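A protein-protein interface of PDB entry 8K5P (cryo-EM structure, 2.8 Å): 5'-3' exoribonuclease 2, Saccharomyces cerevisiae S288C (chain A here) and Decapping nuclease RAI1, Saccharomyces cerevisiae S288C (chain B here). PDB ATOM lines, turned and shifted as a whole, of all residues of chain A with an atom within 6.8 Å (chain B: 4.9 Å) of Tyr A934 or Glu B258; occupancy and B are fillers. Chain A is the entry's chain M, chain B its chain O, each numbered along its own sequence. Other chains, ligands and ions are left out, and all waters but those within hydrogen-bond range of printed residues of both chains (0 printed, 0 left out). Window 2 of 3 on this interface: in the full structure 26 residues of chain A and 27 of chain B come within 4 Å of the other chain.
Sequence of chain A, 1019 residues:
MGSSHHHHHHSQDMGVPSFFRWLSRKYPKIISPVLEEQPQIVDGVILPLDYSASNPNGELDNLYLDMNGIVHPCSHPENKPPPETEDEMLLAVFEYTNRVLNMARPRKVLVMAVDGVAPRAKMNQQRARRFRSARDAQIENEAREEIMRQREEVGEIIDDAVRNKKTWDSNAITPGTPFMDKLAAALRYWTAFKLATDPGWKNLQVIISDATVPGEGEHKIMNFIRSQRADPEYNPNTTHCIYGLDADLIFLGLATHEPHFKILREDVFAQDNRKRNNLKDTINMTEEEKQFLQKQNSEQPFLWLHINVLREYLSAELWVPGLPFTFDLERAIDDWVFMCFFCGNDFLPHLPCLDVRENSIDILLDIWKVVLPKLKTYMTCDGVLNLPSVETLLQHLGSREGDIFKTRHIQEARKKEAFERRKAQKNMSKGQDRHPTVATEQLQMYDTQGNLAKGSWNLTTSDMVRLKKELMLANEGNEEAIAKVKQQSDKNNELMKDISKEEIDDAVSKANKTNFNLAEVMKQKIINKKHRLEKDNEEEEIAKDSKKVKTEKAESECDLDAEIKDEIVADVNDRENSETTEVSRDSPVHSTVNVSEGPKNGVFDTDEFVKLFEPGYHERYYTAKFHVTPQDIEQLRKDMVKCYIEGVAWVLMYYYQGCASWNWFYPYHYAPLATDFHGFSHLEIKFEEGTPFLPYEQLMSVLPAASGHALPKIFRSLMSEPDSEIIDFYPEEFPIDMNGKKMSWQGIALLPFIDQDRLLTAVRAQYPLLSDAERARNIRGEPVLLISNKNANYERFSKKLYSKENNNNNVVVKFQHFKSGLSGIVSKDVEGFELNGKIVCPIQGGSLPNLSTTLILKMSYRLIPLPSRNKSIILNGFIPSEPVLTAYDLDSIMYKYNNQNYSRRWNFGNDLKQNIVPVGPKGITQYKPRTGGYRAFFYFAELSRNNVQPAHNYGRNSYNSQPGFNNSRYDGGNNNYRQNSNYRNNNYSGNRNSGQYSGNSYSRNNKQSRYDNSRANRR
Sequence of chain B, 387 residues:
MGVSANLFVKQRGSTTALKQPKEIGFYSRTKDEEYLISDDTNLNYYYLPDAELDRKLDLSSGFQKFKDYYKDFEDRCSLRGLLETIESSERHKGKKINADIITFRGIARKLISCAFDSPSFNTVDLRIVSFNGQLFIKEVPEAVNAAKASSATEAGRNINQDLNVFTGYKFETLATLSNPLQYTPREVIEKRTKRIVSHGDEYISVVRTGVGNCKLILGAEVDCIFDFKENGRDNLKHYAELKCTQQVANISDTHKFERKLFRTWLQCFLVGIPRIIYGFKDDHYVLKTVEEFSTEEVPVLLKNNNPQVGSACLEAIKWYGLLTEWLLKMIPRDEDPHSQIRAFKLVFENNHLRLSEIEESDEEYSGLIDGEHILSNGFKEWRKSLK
The side-chain carboxylate (OE1) of Glu B258 is in hydrogen-bond range of the side-chain amide nitrogen (ND2) of Asn B306 (2.7 Å).
Of the printed residues of chain B, Gly A933 touches Val B248 (3.6 Å). Tyr A934 touches just these residues of chain B: Phe B257, Glu B258, Leu B261, Phe B293, Leu B301 and Asn B305. Printed residues of chain B within 4 Å of Arg A935: Phe B293. Printed residues of chain A within 4 Å of Phe B257: Tyr A934. Glu B258 touches just one residue of chain A: Tyr A934 (3.4 Å). Of the printed residues of chain A, Leu B301 touches Tyr A934 (3.5 Å). Of the printed residues of chain A, Asn B305 touches Tyr A934 (3.1 Å). The nearest residue of chain B that does not touch Tyr A934 is Thr B254 (4.4 Å). The nearest residue of chain A that does not touch Glu B258 is Phe A938 (5.9 Å). The nearest printed residue of chain A that does not touch Val B248 is Phe A937 (4.4 Å).
Of the 16 printed residues of chain B, 7 touch a printed residue of chain A. Hydrophobic or aromatic side chains of chain B that line the printed part of chain A: Val B248, Phe B257, Leu B261, Phe B293 and Leu B301. Of the 9 printed residues of chain A, 4 touch a printed residue of chain B. Among the printed residues, 9 pairs touch across the chains. Among the printed residues, no Asp or Glu carboxylate lies within 4 Å of a Lys or Arg side-chain nitrogen of the other chain.
OH of Tyr A934 is in hydrogen-bond range of ND2 of Asn B305 (3.1 Å).
Among the printed residues, pairs that only touch across the chains: Arg A935 with Phe B293 (3.3 Å), Tyr A934 with Glu B258 (3.4 Å), Tyr A934 with Leu B261 (3.4 Å), Tyr A934 with Phe B257 (3.5 Å), Tyr A934 with Leu B301 (3.5 Å), Gly A932 with Val B248 (3.6 Å), Gly A933 with Val B248 (3.6 Å) and Tyr A934 with Phe B293 (3.6 Å).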
ATOM      1  N   THR A 931     -20.677  -4.664   6.886  1.00  0.00           N
ATOM      2  CA  THR A 931     -21.191  -5.039   5.572  1.00  0.00           C
ATOM      3  C   THR A 931     -20.046  -5.406   4.634  1.00  0.00           C
ATOM      4  O   THR A 931     -19.335  -6.386   4.874  1.00  0.00           O
ATOM      5  CB  THR A 931     -22.035  -3.911   4.970  1.00  0.00           C
ATOM      6  OG1 THR A 931     -21.178  -2.849   4.530  1.00  0.00           O
ATOM      7  CG2 THR A 931     -23.019  -3.372   5.999  1.00  0.00           C
ATOM      8  N   GLY A 932     -19.860  -4.622   3.575  1.00  0.00           N
ATOM      9  CA  GLY A 932     -18.731  -4.838   2.683  1.00  0.00           C
ATOM     10  C   GLY A 932     -18.769  -6.209   2.038  1.00  0.00           C
ATOM     11  O   GLY A 932     -19.786  -6.633   1.480  1.00  0.00           O
ATOM     12  N   GLY A 933     -17.646  -6.915   2.112  1.00  0.00           N
ATOM     13  CA  GLY A 933     -17.564  -8.239   1.533  1.00  0.00           C
ATOM     14  C   GLY A 933     -16.150  -8.778   1.611  1.00  0.00           C
ATOM     15  O   GLY A 933     -15.286  -8.222   2.295  1.00  0.00           O
ATOM     16  N   TYR A 934     -15.939  -9.880   0.889  1.00  0.00           N
ATOM     17  CA  TYR A 934     -14.662 -10.585   0.849  1.00  0.00           C
ATOM     18  C   TYR A 934     -14.200 -10.987   2.243  1.00  0.00           C
ATOM     19  O   TYR A 934     -14.641 -12.010   2.775  1.00  0.00           O
ATOM     20  CB  TYR A 934     -13.591  -9.740   0.160  1.00  0.00           C
ATOM     21  CG  TYR A 934     -12.740 -10.539  -0.796  1.00  0.00           C
ATOM     22  CD1 TYR A 934     -13.312 -11.203  -1.872  1.00  0.00           C
ATOM     23  CD2 TYR A 934     -11.370 -10.649  -0.611  1.00  0.00           C
ATOM     24  CE1 TYR A 934     -12.541 -11.942  -2.746  1.00  0.00           C
ATOM     25  CE2 TYR A 934     -10.591 -11.388  -1.479  1.00  0.00           C
ATOM     26  CZ  TYR A 934     -11.181 -12.031  -2.545  1.00  0.00           C
ATOM     27  OH  TYR A 934     -10.407 -12.767  -3.413  1.00  0.00           O
ATOM     28  N   ARG A 935     -13.295 -10.202   2.835  1.00  0.00           N
ATOM     29  CA  ARG A 935     -12.851 -10.493   4.195  1.00  0.00           C
ATOM     30  C   ARG A 935     -14.003 -10.381   5.183  1.00  0.00           C
ATOM     31  O   ARG A 935     -14.165 -11.235   6.064  1.00  0.00           O
ATOM     32  CB  ARG A 935     -11.710  -9.553   4.586  1.00  0.00           C
ATOM     33  CG  ARG A 935     -11.065  -9.885   5.921  1.00  0.00           C
ATOM     34  CD  ARG A 935      -9.640  -9.360   5.993  1.00  0.00           C
ATOM     35  NE  ARG A 935      -9.507  -8.053   5.363  1.00  0.00           N
ATOM     36  CZ  ARG A 935      -8.484  -7.690   4.600  1.00  0.00           C
ATOM     37  NH1 ARG A 935      -7.481  -8.515   4.350  1.00  0.00           N
ATOM     38  NH2 ARG A 935      -8.468  -6.467   4.076  1.00  0.00           N
ATOM     39  N   ALA A 936     -14.825  -9.338   5.044  1.00  0.00           N
ATOM     40  CA  ALA A 936     -15.989  -9.193   5.911  1.00  0.00           C
ATOM     41  C   ALA A 936     -17.002 -10.303   5.666  1.00  0.00           C
ATOM     42  O   ALA A 936     -17.640 -10.787   6.607  1.00  0.00           O
ATOM     43  CB  ALA A 936     -16.628  -7.821   5.707  1.00  0.00           C
ATOM     44  N   PHE A 937     -17.167 -10.717   4.407  1.00  0.00           N
ATOM     45  CA  PHE A 937     -18.067 -11.827   4.105  1.00  0.00           C
ATOM     46  C   PHE A 937     -17.588 -13.118   4.760  1.00  0.00           C
ATOM     47  O   PHE A 937     -18.391 -13.872   5.324  1.00  0.00           O
ATOM     48  CB  PHE A 937     -18.185 -12.003   2.591  1.00  0.00           C
ATOM     49  CG  PHE A 937     -19.453 -12.679   2.156  1.00  0.00           C
ATOM     50  CD1 PHE A 937     -20.684 -12.086   2.386  1.00  0.00           C
ATOM     51  CD2 PHE A 937     -19.415 -13.906   1.515  1.00  0.00           C
ATOM     52  CE1 PHE A 937     -21.853 -12.704   1.985  1.00  0.00           C
ATOM     53  CE2 PHE A 937     -20.581 -14.530   1.112  1.00  0.00           C
ATOM     54  CZ  PHE A 937     -21.801 -13.929   1.347  1.00  0.00           C
ATOM     55  N   PHE A 938     -16.282 -13.385   4.697  1.00  0.00           N
ATOM     56  CA  PHE A 938     -15.734 -14.573   5.344  1.00  0.00           C
ATOM     57  C   PHE A 938     -15.889 -14.496   6.857  1.00  0.00           C
ATOM     58  O   PHE A 938     -16.186 -15.503   7.511  1.00  0.00           O
ATOM     59  CB  PHE A 938     -14.264 -14.747   4.963  1.00  0.00           C
ATOM     60  CG  PHE A 938     -14.046 -15.070   3.512  1.00  0.00           C
ATOM     61  CD1 PHE A 938     -15.030 -15.706   2.774  1.00  0.00           C
ATOM     62  CD2 PHE A 938     -12.854 -14.740   2.887  1.00  0.00           C
ATOM     63  CE1 PHE A 938     -14.831 -16.004   1.438  1.00  0.00           C
ATOM     64  CE2 PHE A 938     -12.650 -15.035   1.553  1.00  0.00           C
ATOM     65  CZ  PHE A 938     -13.639 -15.668   0.828  1.00  0.00           C
ATOM     66  N   TYR A 939     -15.683 -13.310   7.433  1.00  0.00           N
ATOM     67  CA  TYR A 939     -15.874 -13.142   8.871  1.00  0.00           C
ATOM     68  C   TYR A 939     -17.322 -13.404   9.265  1.00  0.00           C
ATOM     69  O   TYR A 939     -17.589 -14.077  10.268  1.00  0.00           O
ATOM     70  CB  TYR A 939     -15.422 -11.740   9.294  1.00  0.00           C
ATOM     71  CG  TYR A 939     -16.075 -11.190  10.548  1.00  0.00           C
ATOM     72  CD1 TYR A 939     -15.437 -11.282  11.778  1.00  0.00           C
ATOM     73  CD2 TYR A 939     -17.298 -10.528  10.494  1.00  0.00           C
ATOM     74  CE1 TYR A 939     -16.018 -10.772  12.925  1.00  0.00           C
ATOM     75  CE2 TYR A 939     -17.885 -10.016  11.634  1.00  0.00           C
ATOM     76  CZ  TYR A 939     -17.240 -10.138  12.846  1.00  0.00           C
ATOM     77  OH  TYR A 939     -17.819  -9.626  13.984  1.00  0.00           O
ATOM     78  N   VAL B 248     -20.930  -6.609  -2.256  1.00  0.00           N
ATOM     79  CA  VAL B 248     -21.170  -7.972  -2.710  1.00  0.00           C
ATOM     80  C   VAL B 248     -22.471  -8.470  -2.098  1.00  0.00           C
ATOM     81  O   VAL B 248     -22.882  -8.033  -1.017  1.00  0.00           O
ATOM     82  CB  VAL B 248     -20.000  -8.922  -2.366  1.00  0.00           C
ATOM     83  CG1 VAL B 248     -18.668  -8.286  -2.741  1.00  0.00           C
ATOM     84  CG2 VAL B 248     -20.022  -9.297  -0.893  1.00  0.00           C
ATOM     85  N   THR B 254     -19.115 -11.784  -5.552  1.00  0.00           N
ATOM     86  CA  THR B 254     -17.804 -12.152  -5.026  1.00  0.00           C
ATOM     87  C   THR B 254     -16.803 -12.367  -6.154  1.00  0.00           C
ATOM     88  O   THR B 254     -15.645 -11.947  -6.055  1.00  0.00           O
ATOM     89  CB  THR B 254     -17.916 -13.406  -4.159  1.00  0.00           C
ATOM     90  OG1 THR B 254     -18.960 -13.230  -3.194  1.00  0.00           O
ATOM     91  CG2 THR B 254     -16.605 -13.671  -3.435  1.00  0.00           C
ATOM     92  N   HIS B 255     -17.231 -13.018  -7.238  1.00  0.00           N
ATOM     93  CA  HIS B 255     -16.347 -13.216  -8.383  1.00  0.00           C
ATOM     94  C   HIS B 255     -16.020 -11.893  -9.065  1.00  0.00           C
ATOM     95  O   HIS B 255     -14.894 -11.689  -9.531  1.00  0.00           O
ATOM     96  CB  HIS B 255     -16.981 -14.190  -9.375  1.00  0.00           C
ATOM     97  CG  HIS B 255     -15.993 -14.858 -10.281  1.00  0.00           C
ATOM     98  ND1 HIS B 255     -15.310 -14.177 -11.266  1.00  0.00           N
ATOM     99  CD2 HIS B 255     -15.574 -16.143 -10.352  1.00  0.00           C
ATOM    100  CE1 HIS B 255     -14.511 -15.014 -11.904  1.00  0.00           C
ATOM    101  NE2 HIS B 255     -14.653 -16.214 -11.368  1.00  0.00           N
ATOM    102  N   LYS B 256     -16.996 -10.985  -9.144  1.00  0.00           N
ATOM    103  CA  LYS B 256     -16.724  -9.660  -9.697  1.00  0.00           C
ATOM    104  C   LYS B 256     -15.703  -8.909  -8.847  1.00  0.00           C
ATOM    105  O   LYS B 256     -14.792  -8.258  -9.379  1.00  0.00           O
ATOM    106  CB  LYS B 256     -18.022  -8.862  -9.811  1.00  0.00           C
ATOM    107  CG  LYS B 256     -18.992  -9.400 -10.849  1.00  0.00           C
ATOM    108  CD  LYS B 256     -20.416  -8.947 -10.565  1.00  0.00           C
ATOM    109  CE  LYS B 256     -20.643  -7.515 -11.023  1.00  0.00           C
ATOM    110  NZ  LYS B 256     -20.453  -6.539  -9.914  1.00  0.00           N
ATOM    111  N   PHE B 257     -15.840  -8.990  -7.522  1.00  0.00           N
ATOM    112  CA  PHE B 257     -14.863  -8.369  -6.634  1.00  0.00           C
ATOM    113  C   PHE B 257     -13.494  -9.019  -6.787  1.00  0.00           C
ATOM    114  O   PHE B 257     -12.466  -8.340  -6.713  1.00  0.00           O
ATOM    115  CB  PHE B 257     -15.341  -8.452  -5.185  1.00  0.00           C
ATOM    116  CG  PHE B 257     -14.613  -7.530  -4.253  1.00  0.00           C
ATOM    117  CD1 PHE B 257     -14.562  -6.169  -4.504  1.00  0.00           C
ATOM    118  CD2 PHE B 257     -13.978  -8.022  -3.124  1.00  0.00           C
ATOM    119  CE1 PHE B 257     -13.892  -5.317  -3.647  1.00  0.00           C
ATOM    120  CE2 PHE B 257     -13.307  -7.174  -2.264  1.00  0.00           C
ATOM    121  CZ  PHE B 257     -13.264  -5.820  -2.526  1.00  0.00           C
ATOM    122  N   GLU B 258     -13.463 -10.338  -6.995  1.00  0.00           N
ATOM    123  CA  GLU B 258     -12.200 -11.023  -7.246  1.00  0.00           C
ATOM    124  C   GLU B 258     -11.549 -10.524  -8.529  1.00  0.00           C
ATOM    125  O   GLU B 258     -10.329 -10.334  -8.582  1.00  0.00           O
ATOM    126  CB  GLU B 258     -12.425 -12.534  -7.319  1.00  0.00           C
ATOM    127  CG  GLU B 258     -12.612 -13.208  -5.972  1.00  0.00           C
ATOM    128  CD  GLU B 258     -13.094 -14.640  -6.099  1.00  0.00           C
ATOM    129  OE1 GLU B 258     -13.268 -15.110  -7.244  1.00  0.00           O
ATOM    130  OE2 GLU B 258     -13.299 -15.295  -5.056  1.00  0.00           O
ATOM    131  N   ARG B 259     -12.348 -10.316  -9.577  1.00  0.00           N
ATOM    132  CA  ARG B 259     -11.811  -9.784 -10.826  1.00  0.00           C
ATOM    133  C   ARG B 259     -11.259  -8.376 -10.636  1.00  0.00           C
ATOM    134  O   ARG B 259     -10.182  -8.046 -11.149  1.00  0.00           O
ATOM    135  CB  ARG B 259     -12.889  -9.796 -11.909  1.00  0.00           C
ATOM    136  CG  ARG B 259     -13.292 -11.187 -12.370  1.00  0.00           C
ATOM    137  CD  ARG B 259     -14.347 -11.121 -13.463  1.00  0.00           C
ATOM    138  NE  ARG B 259     -13.986 -10.175 -14.513  1.00  0.00           N
ATOM    139  CZ  ARG B 259     -13.235 -10.474 -15.564  1.00  0.00           C
ATOM    140  NH1 ARG B 259     -12.743 -11.690 -15.739  1.00  0.00           N
ATOM    141  NH2 ARG B 259     -12.970  -9.530 -16.462  1.00  0.00           N
ATOM    142  N   LYS B 260     -11.986  -7.530  -9.901  1.00  0.00           N
ATOM    143  CA  LYS B 260     -11.496  -6.180  -9.631  1.00  0.00           C
ATOM    144  C   LYS B 260     -10.204  -6.216  -8.821  1.00  0.00           C
ATOM    145  O   LYS B 260      -9.275  -5.436  -9.077  1.00  0.00           O
ATOM    146  CB  LYS B 260     -12.566  -5.367  -8.903  1.00  0.00           C
ATOM    147  CG  LYS B 260     -13.846  -5.168  -9.698  1.00  0.00           C
ATOM    148  CD  LYS B 260     -13.556  -4.636 -11.093  1.00  0.00           C
ATOM    149  CE  LYS B 260     -13.301  -3.138 -11.070  1.00  0.00           C
ATOM    150  NZ  LYS B 260     -14.531  -2.370 -10.730  1.00  0.00           N
ATOM    151  N   LEU B 261     -10.132  -7.113  -7.835  1.00  0.00           N
ATOM    152  CA  LEU B 261      -8.912  -7.268  -7.050  1.00  0.00           C
ATOM    153  C   LEU B 261      -7.756  -7.731  -7.923  1.00  0.00           C
ATOM    154  O   LEU B 261      -6.625  -7.269  -7.760  1.00  0.00           O
ATOM    155  CB  LEU B 261      -9.143  -8.255  -5.905  1.00  0.00           C
ATOM    156  CG  LEU B 261      -9.548  -7.699  -4.537  1.00  0.00           C
ATOM    157  CD1 LEU B 261     -10.523  -6.545  -4.671  1.00  0.00           C
ATOM    158  CD2 LEU B 261     -10.146  -8.797  -3.684  1.00  0.00           C
ATOM    159  N   PHE B 262      -8.022  -8.653  -8.848  1.00  0.00           N
ATOM    160  CA  PHE B 262      -6.989  -9.103  -9.775  1.00  0.00           C
ATOM    161  C   PHE B 262      -6.481  -7.946 -10.625  1.00  0.00           C
ATOM    162  O   PHE B 262      -5.268  -7.774 -10.803  1.00  0.00           O
ATOM    163  CB  PHE B 262      -7.541 -10.228 -10.654  1.00  0.00           C
ATOM    164  CG  PHE B 262      -6.698 -10.534 -11.861  1.00  0.00           C
ATOM    165  CD1 PHE B 262      -5.578 -11.341 -11.754  1.00  0.00           C
ATOM    166  CD2 PHE B 262      -7.036 -10.027 -13.105  1.00  0.00           C
ATOM    167  CE1 PHE B 262      -4.806 -11.628 -12.864  1.00  0.00           C
ATOM    168  CE2 PHE B 262      -6.267 -10.309 -14.218  1.00  0.00           C
ATOM    169  CZ  PHE B 262      -5.150 -11.111 -14.096  1.00  0.00           C
ATOM    170  N   PHE B 293      -5.884  -3.395   1.354  1.00  0.00           N
ATOM    171  CA  PHE B 293      -5.396  -4.696   0.901  1.00  0.00           C
ATOM    172  C   PHE B 293      -3.901  -4.574   0.626  1.00  0.00           C
ATOM    173  O   PHE B 293      -3.496  -4.111  -0.445  1.00  0.00           O
ATOM    174  CB  PHE B 293      -6.152  -5.167  -0.337  1.00  0.00           C
ATOM    175  CG  PHE B 293      -7.286  -6.103  -0.036  1.00  0.00           C
ATOM    176  CD1 PHE B 293      -7.125  -7.139   0.868  1.00  0.00           C
ATOM    177  CD2 PHE B 293      -8.514  -5.947  -0.658  1.00  0.00           C
ATOM    178  CE1 PHE B 293      -8.167  -8.002   1.147  1.00  0.00           C
ATOM    179  CE2 PHE B 293      -9.560  -6.807  -0.383  1.00  0.00           C
ATOM    180  CZ  PHE B 293      -9.387  -7.836   0.520  1.00  0.00           C
ATOM    181  N   LEU B 301      -4.647 -14.893  -1.052  1.00  0.00           N
ATOM    182  CA  LEU B 301      -6.086 -14.717  -0.903  1.00  0.00           C
ATOM    183  C   LEU B 301      -6.831 -15.177  -2.152  1.00  0.00           C
ATOM    184  O   LEU B 301      -7.945 -15.704  -2.058  1.00  0.00           O
ATOM    185  CB  LEU B 301      -6.402 -13.256  -0.585  1.00  0.00           C
ATOM    186  CG  LEU B 301      -7.807 -12.940  -0.069  1.00  0.00           C
ATOM    187  CD1 LEU B 301      -8.337 -14.066   0.808  1.00  0.00           C
ATOM    188  CD2 LEU B 301      -7.803 -11.624   0.694  1.00  0.00           C
ATOM    189  N   LEU B 302      -6.244 -14.970  -3.332  1.00  0.00           N
ATOM    190  CA  LEU B 302      -6.847 -15.516  -4.542  1.00  0.00           C
ATOM    191  C   LEU B 302      -6.522 -16.995  -4.720  1.00  0.00           C
ATOM    192  O   LEU B 302      -7.273 -17.714  -5.387  1.00  0.00           O
ATOM    193  CB  LEU B 302      -6.405 -14.721  -5.774  1.00  0.00           C
ATOM    194  CG  LEU B 302      -4.916 -14.445  -5.987  1.00  0.00           C
ATOM    195  CD1 LEU B 302      -4.294 -15.475  -6.919  1.00  0.00           C
ATOM    196  CD2 LEU B 302      -4.706 -13.037  -6.525  1.00  0.00           C
ATOM    197  N   ASN B 305      -9.125 -19.694  -3.166  1.00  0.00           N
ATOM    198  CA  ASN B 305     -10.391 -19.349  -3.800  1.00  0.00           C
ATOM    199  C   ASN B 305     -10.584 -20.291  -4.984  1.00  0.00           C
ATOM    200  O   ASN B 305      -9.959 -21.354  -5.052  1.00  0.00           O
ATOM    201  CB  ASN B 305     -10.409 -17.864  -4.201  1.00  0.00           C
ATOM    202  CG  ASN B 305     -10.854 -16.960  -3.069  1.00  0.00           C
ATOM    203  OD1 ASN B 305     -11.830 -17.249  -2.375  1.00  0.00           O
ATOM    204  ND2 ASN B 305     -10.143 -15.855  -2.879  1.00  0.00           N
ATOM    205  N   ASN B 306     -11.460 -19.911  -5.912  1.00  0.00           N
ATOM    206  CA  ASN B 306     -11.688 -20.723  -7.095  1.00  0.00           C
ATOM    207  C   ASN B 306     -10.394 -20.854  -7.899  1.00  0.00           C
ATOM    208  O   ASN B 306      -9.571 -19.934  -7.923  1.00  0.00           O
ATOM    209  CB  ASN B 306     -12.787 -20.111  -7.962  1.00  0.00           C
ATOM    210  CG  ASN B 306     -12.438 -18.719  -8.451  1.00  0.00           C
ATOM    211  OD1 ASN B 306     -11.788 -18.557  -9.485  1.00  0.00           O
ATOM    212  ND2 ASN B 306     -12.870 -17.706  -7.710  1.00  0.00           N
ATOM    213  N   VAL B 309      -9.165 -17.805 -10.521  1.00  0.00           N
ATOM    214  CA  VAL B 309      -8.461 -16.626 -10.026  1.00  0.00           C
ATOM    215  C   VAL B 309      -7.106 -17.010  -9.442  1.00  0.00           C
ATOM    216  O   VAL B 309      -6.162 -16.212  -9.472  1.00  0.00           O
ATOM    217  CB  VAL B 309      -9.327 -15.863  -9.004  1.00  0.00           C
ATOM    218  CG1 VAL B 309     -10.628 -15.409  -9.648  1.00  0.00           C
ATOM    219  CG2 VAL B 309      -9.603 -16.720  -7.778  1.00  0.00           C
